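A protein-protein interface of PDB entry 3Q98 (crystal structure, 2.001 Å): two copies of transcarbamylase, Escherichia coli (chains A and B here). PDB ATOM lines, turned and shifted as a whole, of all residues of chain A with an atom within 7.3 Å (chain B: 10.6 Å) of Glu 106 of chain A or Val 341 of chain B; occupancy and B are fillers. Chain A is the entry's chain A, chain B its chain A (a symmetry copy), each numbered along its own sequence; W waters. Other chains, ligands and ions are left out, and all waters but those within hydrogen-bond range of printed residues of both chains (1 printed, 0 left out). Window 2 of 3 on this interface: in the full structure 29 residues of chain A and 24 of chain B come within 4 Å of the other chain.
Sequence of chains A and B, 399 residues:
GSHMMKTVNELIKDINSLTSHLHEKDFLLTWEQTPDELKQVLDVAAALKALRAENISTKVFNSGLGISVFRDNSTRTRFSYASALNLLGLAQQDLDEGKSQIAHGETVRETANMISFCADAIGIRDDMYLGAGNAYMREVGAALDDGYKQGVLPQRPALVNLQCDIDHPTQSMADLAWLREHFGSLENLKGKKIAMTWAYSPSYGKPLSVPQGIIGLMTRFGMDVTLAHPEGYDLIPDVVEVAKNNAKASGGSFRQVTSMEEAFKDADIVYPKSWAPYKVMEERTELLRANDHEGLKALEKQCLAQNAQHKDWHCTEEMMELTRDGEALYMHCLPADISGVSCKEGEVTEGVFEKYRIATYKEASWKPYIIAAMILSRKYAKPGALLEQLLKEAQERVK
The side-chain carboxylate (OE2) of Glu 110 of chain A is in salt-bridge range of the guanidinium group (NE) of Arg 109 of chain A (3.3 Å).
N of Ile 338 of chain B is in hydrogen-bond range of OG of Ser 342 of chain B (3.3 Å).
O of His 104 of chain A sits at hydrogen-bond distance from OG1 of Thr 107 of chain A.
Among the printed residues, merely in contact across the chains: Glu 106 of chain A with Val 341 of chain B (3.4 Å), Thr 107 of chain A with Ser 342 of chain B (3.9 Å), Arg 109 of chain A with Tyr 361 of chain B (3.9 Å), Glu 110 of chain A with Phe 353 of chain B (3.5 Å) and Glu 110 of chain A with Tyr 361 of chain B (3.7 Å).
No residue of chain B comes within 4 Å of Gly 105 of chain A.
Glu 106 of chain A touches one residue of chain B.
Of chain B, only Ser 342 (3.9 Å) comes within 4 Å of Thr 107 of chain A.
Gly 340 of chain B touches none of the printed residues of chain A.
Val 341 of chain B touches just one residue of chain A: Glu 106 (3.4 Å).
Printed residues of chain A within 4 Å of Phe 353 of chain B: Glu 110.
Printed residues of chain A within 4 Å of Tyr 361 of chain B: Arg 109 and Glu 110.
The nearest residue of chain B that does not touch Glu 106 of chain A is Ser 342 of chain B (5.3 Å).
Of the 23 printed residues of chain B, 4 touch a printed residue of chain A.
Printed residues of chain B that touch a printed residue of chain A: Val 341, Ser 342, Phe 353 and Tyr 361.
Hydrophobic or aromatic side chains of chain B that line the printed part of chain A: Val 341, Phe 353 and Tyr 361.
Among the printed residues, 5 pairs touch across the chains.
Among the printed residues, no Asp or Glu carboxylate lies within 4 Å of a Lys or Arg side-chain nitrogen of the other chain.
No position is printed for both chains.
Water W1 bridges OE2 of Glu 110 of chain A (2.4 Å) and OH of Tyr 361 of chain B (2.8 Å).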
ATOM      1  N   ARG A  71      10.405   7.606  -3.243  1.00  0.00           N
ATOM      2  CA  ARG A  71      10.176   8.116  -1.895  1.00  0.00           C
ATOM      3  C   ARG A  71       9.985   9.637  -1.921  1.00  0.00           C
ATOM      4  O   ARG A  71      10.914  10.390  -1.619  1.00  0.00           O
ATOM      5  CB  ARG A  71      11.334   7.753  -0.961  1.00  0.00           C
ATOM      6  CG  ARG A  71      11.536   6.268  -0.728  1.00  0.00           C
ATOM      7  CD  ARG A  71      12.591   6.043   0.356  1.00  0.00           C
ATOM      8  NE  ARG A  71      12.189   6.642   1.630  1.00  0.00           N
ATOM      9  CZ  ARG A  71      12.992   6.801   2.679  1.00  0.00           C
ATOM     10  NH1 ARG A  71      14.258   6.413   2.618  1.00  0.00           N
ATOM     11  NH2 ARG A  71      12.532   7.354   3.792  1.00  0.00           N
ATOM     12  N   HIS A 104       7.636   3.373   4.896  1.00  0.00           N
ATOM     13  CA  HIS A 104       8.162   2.442   3.901  1.00  0.00           C
ATOM     14  C   HIS A 104       9.633   2.101   4.147  1.00  0.00           C
ATOM     15  O   HIS A 104      10.143   1.113   3.626  1.00  0.00           O
ATOM     16  CB  HIS A 104       7.957   2.989   2.487  1.00  0.00           C
ATOM     17  CG  HIS A 104       8.342   4.428   2.337  1.00  0.00           C
ATOM     18  ND1 HIS A 104       7.537   5.462   2.766  1.00  0.00           N
ATOM     19  CD2 HIS A 104       9.446   5.006   1.807  1.00  0.00           C
ATOM     20  CE1 HIS A 104       8.128   6.615   2.505  1.00  0.00           C
ATOM     21  NE2 HIS A 104       9.288   6.366   1.923  1.00  0.00           N
ATOM     22  N   GLY A 105      10.312   2.917   4.943  1.00  0.00           N
ATOM     23  CA  GLY A 105      11.674   2.614   5.339  1.00  0.00           C
ATOM     24  C   GLY A 105      11.717   1.355   6.184  1.00  0.00           C
ATOM     25  O   GLY A 105      12.610   0.519   6.034  1.00  0.00           O
ATOM     26  N   GLU A 106      10.726   1.207   7.060  1.00  0.00           N
ATOM     27  CA  GLU A 106      10.644   0.076   7.979  1.00  0.00           C
ATOM     28  C   GLU A 106      10.431  -1.269   7.279  1.00  0.00           C
ATOM     29  O   GLU A 106      10.723  -2.331   7.838  1.00  0.00           O
ATOM     30  CB  GLU A 106       9.506   0.304   8.981  1.00  0.00           C
ATOM     31  CG  GLU A 106       9.749   1.434   9.977  1.00  0.00           C
ATOM     32  CD  GLU A 106       9.224   2.787   9.506  1.00  0.00           C
ATOM     33  OE1 GLU A 106       9.074   2.997   8.280  1.00  0.00           O
ATOM     34  OE2 GLU A 106       8.967   3.650  10.376  1.00  0.00           O
ATOM     35  N   THR A 107       9.905  -1.225   6.063  1.00  0.00           N
ATOM     36  CA  THR A 107       9.504  -2.447   5.378  1.00  0.00           C
ATOM     37  C   THR A 107      10.318  -2.643   4.109  1.00  0.00           C
ATOM     38  O   THR A 107      10.045  -3.547   3.324  1.00  0.00           O
ATOM     39  CB  THR A 107       8.009  -2.404   5.012  1.00  0.00           C
ATOM     40  OG1 THR A 107       7.766  -1.315   4.111  1.00  0.00           O
ATOM     41  CG2 THR A 107       7.171  -2.209   6.254  1.00  0.00           C
ATOM     42  N   VAL A 108      11.322  -1.791   3.925  1.00  0.00           N
ATOM     43  CA  VAL A 108      12.108  -1.766   2.702  1.00  0.00           C
ATOM     44  C   VAL A 108      12.647  -3.136   2.285  1.00  0.00           C
ATOM     45  O   VAL A 108      12.676  -3.469   1.101  1.00  0.00           O
ATOM     46  CB  VAL A 108      13.292  -0.770   2.811  1.00  0.00           C
ATOM     47  CG1 VAL A 108      14.071  -0.987   4.100  1.00  0.00           C
ATOM     48  CG2 VAL A 108      14.205  -0.926   1.633  1.00  0.00           C
ATOM     49  N   ARG A 109      13.070  -3.930   3.256  1.00  0.00           N
ATOM     50  CA  ARG A 109      13.712  -5.202   2.953  1.00  0.00           C
ATOM     51  C   ARG A 109      12.739  -6.189   2.303  1.00  0.00           C
ATOM     52  O   ARG A 109      13.086  -6.880   1.346  1.00  0.00           O
ATOM     53  CB  ARG A 109      14.331  -5.800   4.216  1.00  0.00           C
ATOM     54  CG  ARG A 109      14.977  -4.755   5.133  1.00  0.00           C
ATOM     55  CD  ARG A 109      13.963  -4.153   6.135  1.00  0.00           C
ATOM     56  NE  ARG A 109      13.498  -5.146   7.104  1.00  0.00           N
ATOM     57  CZ  ARG A 109      13.938  -5.244   8.358  1.00  0.00           C
ATOM     58  NH1 ARG A 109      14.849  -4.398   8.832  1.00  0.00           N
ATOM     59  NH2 ARG A 109      13.465  -6.194   9.145  1.00  0.00           N
ATOM     60  N   GLU A 110      11.524  -6.255   2.831  1.00  0.00           N
ATOM     61  CA  GLU A 110      10.515  -7.171   2.306  1.00  0.00           C
ATOM     62  C   GLU A 110      10.034  -6.709   0.936  1.00  0.00           C
ATOM     63  O   GLU A 110       9.834  -7.512   0.023  1.00  0.00           O
ATOM     64  CB  GLU A 110       9.338  -7.286   3.276  1.00  0.00           C
ATOM     65  CG  GLU A 110       9.702  -7.913   4.630  1.00  0.00           C
ATOM     66  CD  GLU A 110      10.340  -6.920   5.606  1.00  0.00           C
ATOM     67  OE1 GLU A 110      10.085  -5.706   5.469  1.00  0.00           O
ATOM     68  OE2 GLU A 110      11.076  -7.361   6.522  1.00  0.00           O
ATOM     69  N   TYR A 136      18.544   3.993   3.161  1.00  0.00           N
ATOM     70  CA  TYR A 136      17.472   3.274   2.492  1.00  0.00           C
ATOM     71  C   TYR A 136      17.992   2.396   1.354  1.00  0.00           C
ATOM     72  O   TYR A 136      17.727   1.201   1.318  1.00  0.00           O
ATOM     73  CB  TYR A 136      16.414   4.261   1.990  1.00  0.00           C
ATOM     74  CG  TYR A 136      15.198   3.611   1.368  1.00  0.00           C
ATOM     75  CD1 TYR A 136      14.131   3.187   2.153  1.00  0.00           C
ATOM     76  CD2 TYR A 136      15.108   3.436  -0.005  1.00  0.00           C
ATOM     77  CE1 TYR A 136      13.007   2.596   1.576  1.00  0.00           C
ATOM     78  CE2 TYR A 136      13.998   2.851  -0.589  1.00  0.00           C
ATOM     79  CZ  TYR A 136      12.948   2.433   0.200  1.00  0.00           C
ATOM     80  OH  TYR A 136      11.845   1.842  -0.391  1.00  0.00           O
ATOM     81  N   ARG A 289       6.233  13.102   6.968  1.00  0.00           N
ATOM     82  CA  ARG A 289       6.014  11.799   7.587  1.00  0.00           C
ATOM     83  C   ARG A 289       4.824  11.813   8.548  1.00  0.00           C
ATOM     84  O   ARG A 289       4.236  10.772   8.833  1.00  0.00           O
ATOM     85  CB  ARG A 289       7.274  11.350   8.336  1.00  0.00           C
ATOM     86  CG  ARG A 289       8.416  10.899   7.441  1.00  0.00           C
ATOM     87  CD  ARG A 289       9.730  10.795   8.215  1.00  0.00           C
ATOM     88  NE  ARG A 289       9.626   9.955   9.407  1.00  0.00           N
ATOM     89  CZ  ARG A 289       9.450  10.422  10.642  1.00  0.00           C
ATOM     90  NH1 ARG A 289       9.357  11.729  10.851  1.00  0.00           N
ATOM     91  NH2 ARG A 289       9.369   9.584  11.668  1.00  0.00           N
ATOM     92  N   PRO B 202      -4.648  -4.179  11.807  1.00  0.00           N
ATOM     93  CA  PRO B 202      -5.094  -2.813  12.085  1.00  0.00           C
ATOM     94  C   PRO B 202      -5.938  -2.293  10.936  1.00  0.00           C
ATOM     95  O   PRO B 202      -6.649  -1.308  11.083  1.00  0.00           O
ATOM     96  CB  PRO B 202      -3.780  -2.022  12.155  1.00  0.00           C
ATOM     97  CG  PRO B 202      -2.701  -3.049  12.312  1.00  0.00           C
ATOM     98  CD  PRO B 202      -3.193  -4.252  11.591  1.00  0.00           C
ATOM     99  N   HIS B 314      -2.470 -13.600  17.069  1.00  0.00           N
ATOM    100  CA  HIS B 314      -1.181 -13.000  16.761  1.00  0.00           C
ATOM    101  C   HIS B 314      -0.209 -14.165  16.619  1.00  0.00           C
ATOM    102  O   HIS B 314      -0.078 -14.969  17.535  1.00  0.00           O
ATOM    103  CB  HIS B 314      -0.785 -12.095  17.944  1.00  0.00           C
ATOM    104  CG  HIS B 314       0.450 -11.271  17.721  1.00  0.00           C
ATOM    105  ND1 HIS B 314       0.859 -10.846  16.474  1.00  0.00           N
ATOM    106  CD2 HIS B 314       1.351 -10.768  18.600  1.00  0.00           C
ATOM    107  CE1 HIS B 314       1.964 -10.127  16.592  1.00  0.00           C
ATOM    108  NE2 HIS B 314       2.287 -10.071  17.869  1.00  0.00           N
ATOM    109  N   PRO B 335       2.157  -8.156   1.393  1.00  0.00           N
ATOM    110  CA  PRO B 335       2.844  -7.890   2.664  1.00  0.00           C
ATOM    111  C   PRO B 335       2.087  -8.421   3.869  1.00  0.00           C
ATOM    112  O   PRO B 335       0.875  -8.561   3.831  1.00  0.00           O
ATOM    113  CB  PRO B 335       2.879  -6.349   2.738  1.00  0.00           C
ATOM    114  CG  PRO B 335       2.163  -5.840   1.510  1.00  0.00           C
ATOM    115  CD  PRO B 335       1.399  -6.983   0.925  1.00  0.00           C
ATOM    116  N   ALA B 336       2.810  -8.710   4.942  1.00  0.00           N
ATOM    117  CA  ALA B 336       2.181  -9.054   6.206  1.00  0.00           C
ATOM    118  C   ALA B 336       2.172  -7.819   7.091  1.00  0.00           C
ATOM    119  O   ALA B 336       2.990  -6.916   6.903  1.00  0.00           O
ATOM    120  CB  ALA B 336       2.938 -10.184   6.882  1.00  0.00           C
ATOM    121  N   ASP B 337       1.224  -7.755   8.020  1.00  0.00           N
ATOM    122  CA  ASP B 337       1.266  -6.737   9.064  1.00  0.00           C
ATOM    123  C   ASP B 337       2.161  -7.241  10.179  1.00  0.00           C
ATOM    124  O   ASP B 337       1.760  -8.084  10.979  1.00  0.00           O
ATOM    125  CB  ASP B 337      -0.130  -6.449   9.610  1.00  0.00           C
ATOM    126  CG  ASP B 337      -1.059  -5.902   8.544  1.00  0.00           C
ATOM    127  OD1 ASP B 337      -0.555  -5.235   7.611  1.00  0.00           O
ATOM    128  OD2 ASP B 337      -2.282  -6.146   8.631  1.00  0.00           O
ATOM    129  N   ILE B 338       3.379  -6.722  10.218  1.00  0.00           N
ATOM    130  CA  ILE B 338       4.364  -7.135  11.201  1.00  0.00           C
ATOM    131  C   ILE B 338       4.347  -6.198  12.392  1.00  0.00           C
ATOM    132  O   ILE B 338       4.605  -5.001  12.256  1.00  0.00           O
ATOM    133  CB  ILE B 338       5.766  -7.169  10.573  1.00  0.00           C
ATOM    134  CG1 ILE B 338       5.760  -8.094   9.363  1.00  0.00           C
ATOM    135  CG2 ILE B 338       6.809  -7.625  11.580  1.00  0.00           C
ATOM    136  CD1 ILE B 338       6.997  -7.978   8.511  1.00  0.00           C
ATOM    137  N   SER B 339       4.033  -6.752  13.562  1.00  0.00           N
ATOM    138  CA  SER B 339       3.995  -5.985  14.803  1.00  0.00           C
ATOM    139  C   SER B 339       5.301  -5.243  15.070  1.00  0.00           C
ATOM    140  O   SER B 339       6.383  -5.818  14.958  1.00  0.00           O
ATOM    141  CB  SER B 339       3.678  -6.907  15.987  1.00  0.00           C
ATOM    142  OG  SER B 339       2.398  -7.490  15.819  1.00  0.00           O
ATOM    143  N   GLY B 340       5.183  -3.966  15.426  1.00  0.00           N
ATOM    144  CA  GLY B 340       6.337  -3.147  15.754  1.00  0.00           C
ATOM    145  C   GLY B 340       7.172  -2.752  14.543  1.00  0.00           C
ATOM    146  O   GLY B 340       8.172  -2.057  14.676  1.00  0.00           O
ATOM    147  N   VAL B 341       6.771  -3.204  13.359  1.00  0.00           N
ATOM    148  CA  VAL B 341       7.476  -2.836  12.134  1.00  0.00           C
ATOM    149  C   VAL B 341       6.550  -2.058  11.212  1.00  0.00           C
ATOM    150  O   VAL B 341       6.731  -0.849  11.009  1.00  0.00           O
ATOM    151  CB  VAL B 341       8.008  -4.068  11.380  1.00  0.00           C
ATOM    152  CG1 VAL B 341       8.526  -3.669  10.008  1.00  0.00           C
ATOM    153  CG2 VAL B 341       9.097  -4.756  12.174  1.00  0.00           C
ATOM    154  N   SER B 342       5.558  -2.767  10.669  1.00  0.00           N
ATOM    155  CA  SER B 342       4.559  -2.210   9.761  1.00  0.00           C
ATOM    156  C   SER B 342       3.521  -1.425  10.539  1.00  0.00           C
ATOM    157  O   SER B 342       2.858  -0.539  10.000  1.00  0.00           O
ATOM    158  CB  SER B 342       3.828  -3.337   9.024  1.00  0.00           C
ATOM    159  OG  SER B 342       4.727  -4.294   8.504  1.00  0.00           O
ATOM    160  N   CYS B 343       3.376  -1.777  11.810  1.00  0.00           N
ATOM    161  CA  CYS B 343       2.263  -1.308  12.619  1.00  0.00           C
ATOM    162  C   CYS B 343       2.593  -1.576  14.079  1.00  0.00           C
ATOM    163  O   CYS B 343       3.587  -2.222  14.379  1.00  0.00           O
ATOM    164  CB  CYS B 343       1.003  -2.082  12.228  1.00  0.00           C
ATOM    165  SG  CYS B 343       1.220  -3.873  12.316  1.00  0.00           S
ATOM    166  N   LYS B 344       1.753  -1.095  14.986  1.00  0.00           N
ATOM    167  CA  LYS B 344       1.955  -1.351  16.408  1.00  0.00           C
ATOM    168  C   LYS B 344       1.658  -2.819  16.720  1.00  0.00           C
ATOM    169  O   LYS B 344       2.482  -3.517  17.319  1.00  0.00           O
ATOM    170  CB  LYS B 344       1.082  -0.429  17.273  1.00  0.00           C
ATOM    171  CG  LYS B 344       1.306   1.081  17.051  1.00  0.00           C
ATOM    172  CD  LYS B 344       0.831   1.549  15.661  1.00  0.00           C
ATOM    173  CE  LYS B 344       0.950   3.070  15.469  1.00  0.00           C
ATOM    174  NZ  LYS B 344       0.653   3.461  14.052  1.00  0.00           N
ATOM    175  N   GLU B 345       0.476  -3.276  16.309  1.00  0.00           N
ATOM    176  CA  GLU B 345       0.049  -4.663  16.518  1.00  0.00           C
ATOM    177  C   GLU B 345      -0.494  -5.206  15.209  1.00  0.00           C
ATOM    178  O   GLU B 345      -1.333  -4.566  14.590  1.00  0.00           O
ATOM    179  CB  GLU B 345      -1.054  -4.742  17.579  1.00  0.00           C
ATOM    180  CG  GLU B 345      -0.627  -4.302  18.960  1.00  0.00           C
ATOM    181  CD  GLU B 345      -1.806  -3.925  19.836  1.00  0.00           C
ATOM    182  OE1 GLU B 345      -2.905  -3.701  19.287  1.00  0.00           O
ATOM    183  OE2 GLU B 345      -1.633  -3.844  21.074  1.00  0.00           O
ATOM    184  N   GLY B 346      -0.025  -6.385  14.801  1.00  0.00           N
ATOM    185  CA  GLY B 346      -0.399  -6.962  13.519  1.00  0.00           C
ATOM    186  C   GLY B 346      -0.611  -8.467  13.575  1.00  0.00           C
ATOM    187  O   GLY B 346      -0.994  -9.011  14.612  1.00  0.00           O
ATOM    188  N   GLU B 347      -0.360  -9.135  12.455  1.00  0.00           N
ATOM    189  CA  GLU B 347      -0.677 -10.548  12.293  1.00  0.00           C
ATOM    190  C   GLU B 347       0.445 -11.479  12.744  1.00  0.00           C
ATOM    191  O   GLU B 347       0.196 -12.644  13.029  1.00  0.00           O
ATOM    192  CB  GLU B 347      -0.962 -10.851  10.824  1.00  0.00           C
ATOM    193  CG  GLU B 347      -2.083 -10.039  10.221  1.00  0.00           C
ATOM    194  CD  GLU B 347      -2.060 -10.100   8.717  1.00  0.00           C
ATOM    195  OE1 GLU B 347      -3.005 -10.657   8.128  1.00  0.00           O
ATOM    196  OE2 GLU B 347      -1.074  -9.615   8.120  1.00  0.00           O
ATOM    197  N   VAL B 348       1.672 -10.957  12.792  1.00  0.00           N
ATOM    198  CA  VAL B 348       2.863 -11.767  13.073  1.00  0.00           C
ATOM    199  C   VAL B 348       3.982 -10.907  13.690  1.00  0.00           C
ATOM    200  O   VAL B 348       4.121  -9.736  13.362  1.00  0.00           O
ATOM    201  CB  VAL B 348       3.360 -12.454  11.778  1.00  0.00           C
ATOM    202  CG1 VAL B 348       3.834 -11.394  10.759  1.00  0.00           C
ATOM    203  CG2 VAL B 348       4.457 -13.481  12.076  1.00  0.00           C
ATOM    204  N   THR B 349       4.773 -11.473  14.592  1.00  0.00           N
ATOM    205  CA  THR B 349       5.817 -10.680  15.241  1.00  0.00           C
ATOM    206  C   THR B 349       7.031 -10.570  14.330  1.00  0.00           C
ATOM    207  O   THR B 349       7.214 -11.387  13.433  1.00  0.00           O
ATOM    208  CB  THR B 349       6.282 -11.318  16.558  1.00  0.00           C
ATOM    209  OG1 THR B 349       6.882 -12.583  16.276  1.00  0.00           O
ATOM    210  CG2 THR B 349       5.111 -11.509  17.533  1.00  0.00           C
ATOM    211  N   GLU B 350       7.852  -9.552  14.576  1.00  0.00           N
ATOM    212  CA  GLU B 350       9.111  -9.346  13.863  1.00  0.00           C
ATOM    213  C   GLU B 350      10.003 -10.591  13.858  1.00  0.00           C
ATOM    214  O   GLU B 350      10.587 -10.933  12.831  1.00  0.00           O
ATOM    215  CB  GLU B 350       9.874  -8.168  14.487  1.00  0.00           C
ATOM    216  CG  GLU B 350      10.953  -7.585  13.596  1.00  0.00           C
ATOM    217  CD  GLU B 350      11.453  -6.223  14.074  1.00  0.00           C
ATOM    218  OE1 GLU B 350      10.996  -5.746  15.144  1.00  0.00           O
ATOM    219  OE2 GLU B 350      12.301  -5.634  13.369  1.00  0.00           O
ATOM    220  N   GLY B 351      10.104 -11.258  15.008  1.00  0.00           N
ATOM    221  CA  GLY B 351      10.959 -12.424  15.168  1.00  0.00           C
ATOM    222  C   GLY B 351      10.528 -13.638  14.354  1.00  0.00           C
ATOM    223  O   GLY B 351      11.356 -14.319  13.745  1.00  0.00           O
ATOM    224  N   VAL B 352       9.233 -13.940  14.356  1.00  0.00           N
ATOM    225  CA  VAL B 352       8.730 -15.065  13.566  1.00  0.00           C
ATOM    226  C   VAL B 352       8.883 -14.759  12.075  1.00  0.00           C
ATOM    227  O   VAL B 352       9.243 -15.631  11.279  1.00  0.00           O
ATOM    228  CB  VAL B 352       7.250 -15.405  13.900  1.00  0.00           C
ATOM    229  CG1 VAL B 352       6.686 -16.383  12.894  1.00  0.00           C
ATOM    230  CG2 VAL B 352       7.124 -15.976  15.309  1.00  0.00           C
ATOM    231  N   PHE B 353       8.623 -13.517  11.684  1.00  0.00           N
ATOM    232  CA  PHE B 353       8.764 -13.187  10.271  1.00  0.00           C
ATOM    233  C   PHE B 353      10.224 -13.285   9.804  1.00  0.00           C
ATOM    234  O   PHE B 353      10.498 -13.779   8.709  1.00  0.00           O
ATOM    235  CB  PHE B 353       8.205 -11.804   9.940  1.00  0.00           C
ATOM    236  CG  PHE B 353       8.053 -11.578   8.464  1.00  0.00           C
ATOM    237  CD1 PHE B 353       6.892 -11.956   7.808  1.00  0.00           C
ATOM    238  CD2 PHE B 353       9.091 -11.033   7.725  1.00  0.00           C
ATOM    239  CE1 PHE B 353       6.759 -11.773   6.428  1.00  0.00           C
ATOM    240  CE2 PHE B 353       8.960 -10.851   6.351  1.00  0.00           C
ATOM    241  CZ  PHE B 353       7.790 -11.222   5.710  1.00  0.00           C
ATOM    242  N   GLU B 354      11.158 -12.799  10.618  1.00  0.00           N
ATOM    243  CA  GLU B 354      12.576 -12.885  10.265  1.00  0.00           C
ATOM    244  C   GLU B 354      12.976 -14.346  10.023  1.00  0.00           C
ATOM    245  O   GLU B 354      13.639 -14.663   9.037  1.00  0.00           O
ATOM    246  CB  GLU B 354      13.461 -12.243  11.347  1.00  0.00           C
ATOM    247  CG  GLU B 354      14.967 -12.400  11.101  1.00  0.00           C
ATOM    248  CD  GLU B 354      15.458 -11.654   9.865  1.00  0.00           C
ATOM    249  OE1 GLU B 354      14.932 -10.560   9.576  1.00  0.00           O
ATOM    250  OE2 GLU B 354      16.381 -12.157   9.188  1.00  0.00           O
ATOM    251  N   TYR B 361       9.070 -15.364   0.871  1.00  0.00           N
ATOM    252  CA  TYR B 361       9.551 -14.844  -0.405  1.00  0.00           C
ATOM    253  C   TYR B 361       9.454 -15.904  -1.495  1.00  0.00           C
ATOM    254  O   TYR B 361       9.040 -15.607  -2.617  1.00  0.00           O
ATOM    255  CB  TYR B 361      11.004 -14.391  -0.326  1.00  0.00           C
ATOM    256  CG  TYR B 361      11.316 -13.276   0.643  1.00  0.00           C
ATOM    257  CD1 TYR B 361      10.326 -12.449   1.156  1.00  0.00           C
ATOM    258  CD2 TYR B 361      12.623 -13.041   1.020  1.00  0.00           C
ATOM    259  CE1 TYR B 361      10.636 -11.435   2.049  1.00  0.00           C
ATOM    260  CE2 TYR B 361      12.950 -12.031   1.895  1.00  0.00           C
ATOM    261  CZ  TYR B 361      11.958 -11.230   2.409  1.00  0.00           C
ATOM    262  OH  TYR B 361      12.313 -10.231   3.288  1.00  0.00           O
HETATM  263  O   HOH W   1      12.734  -8.995   5.759  1.00  0.00           O
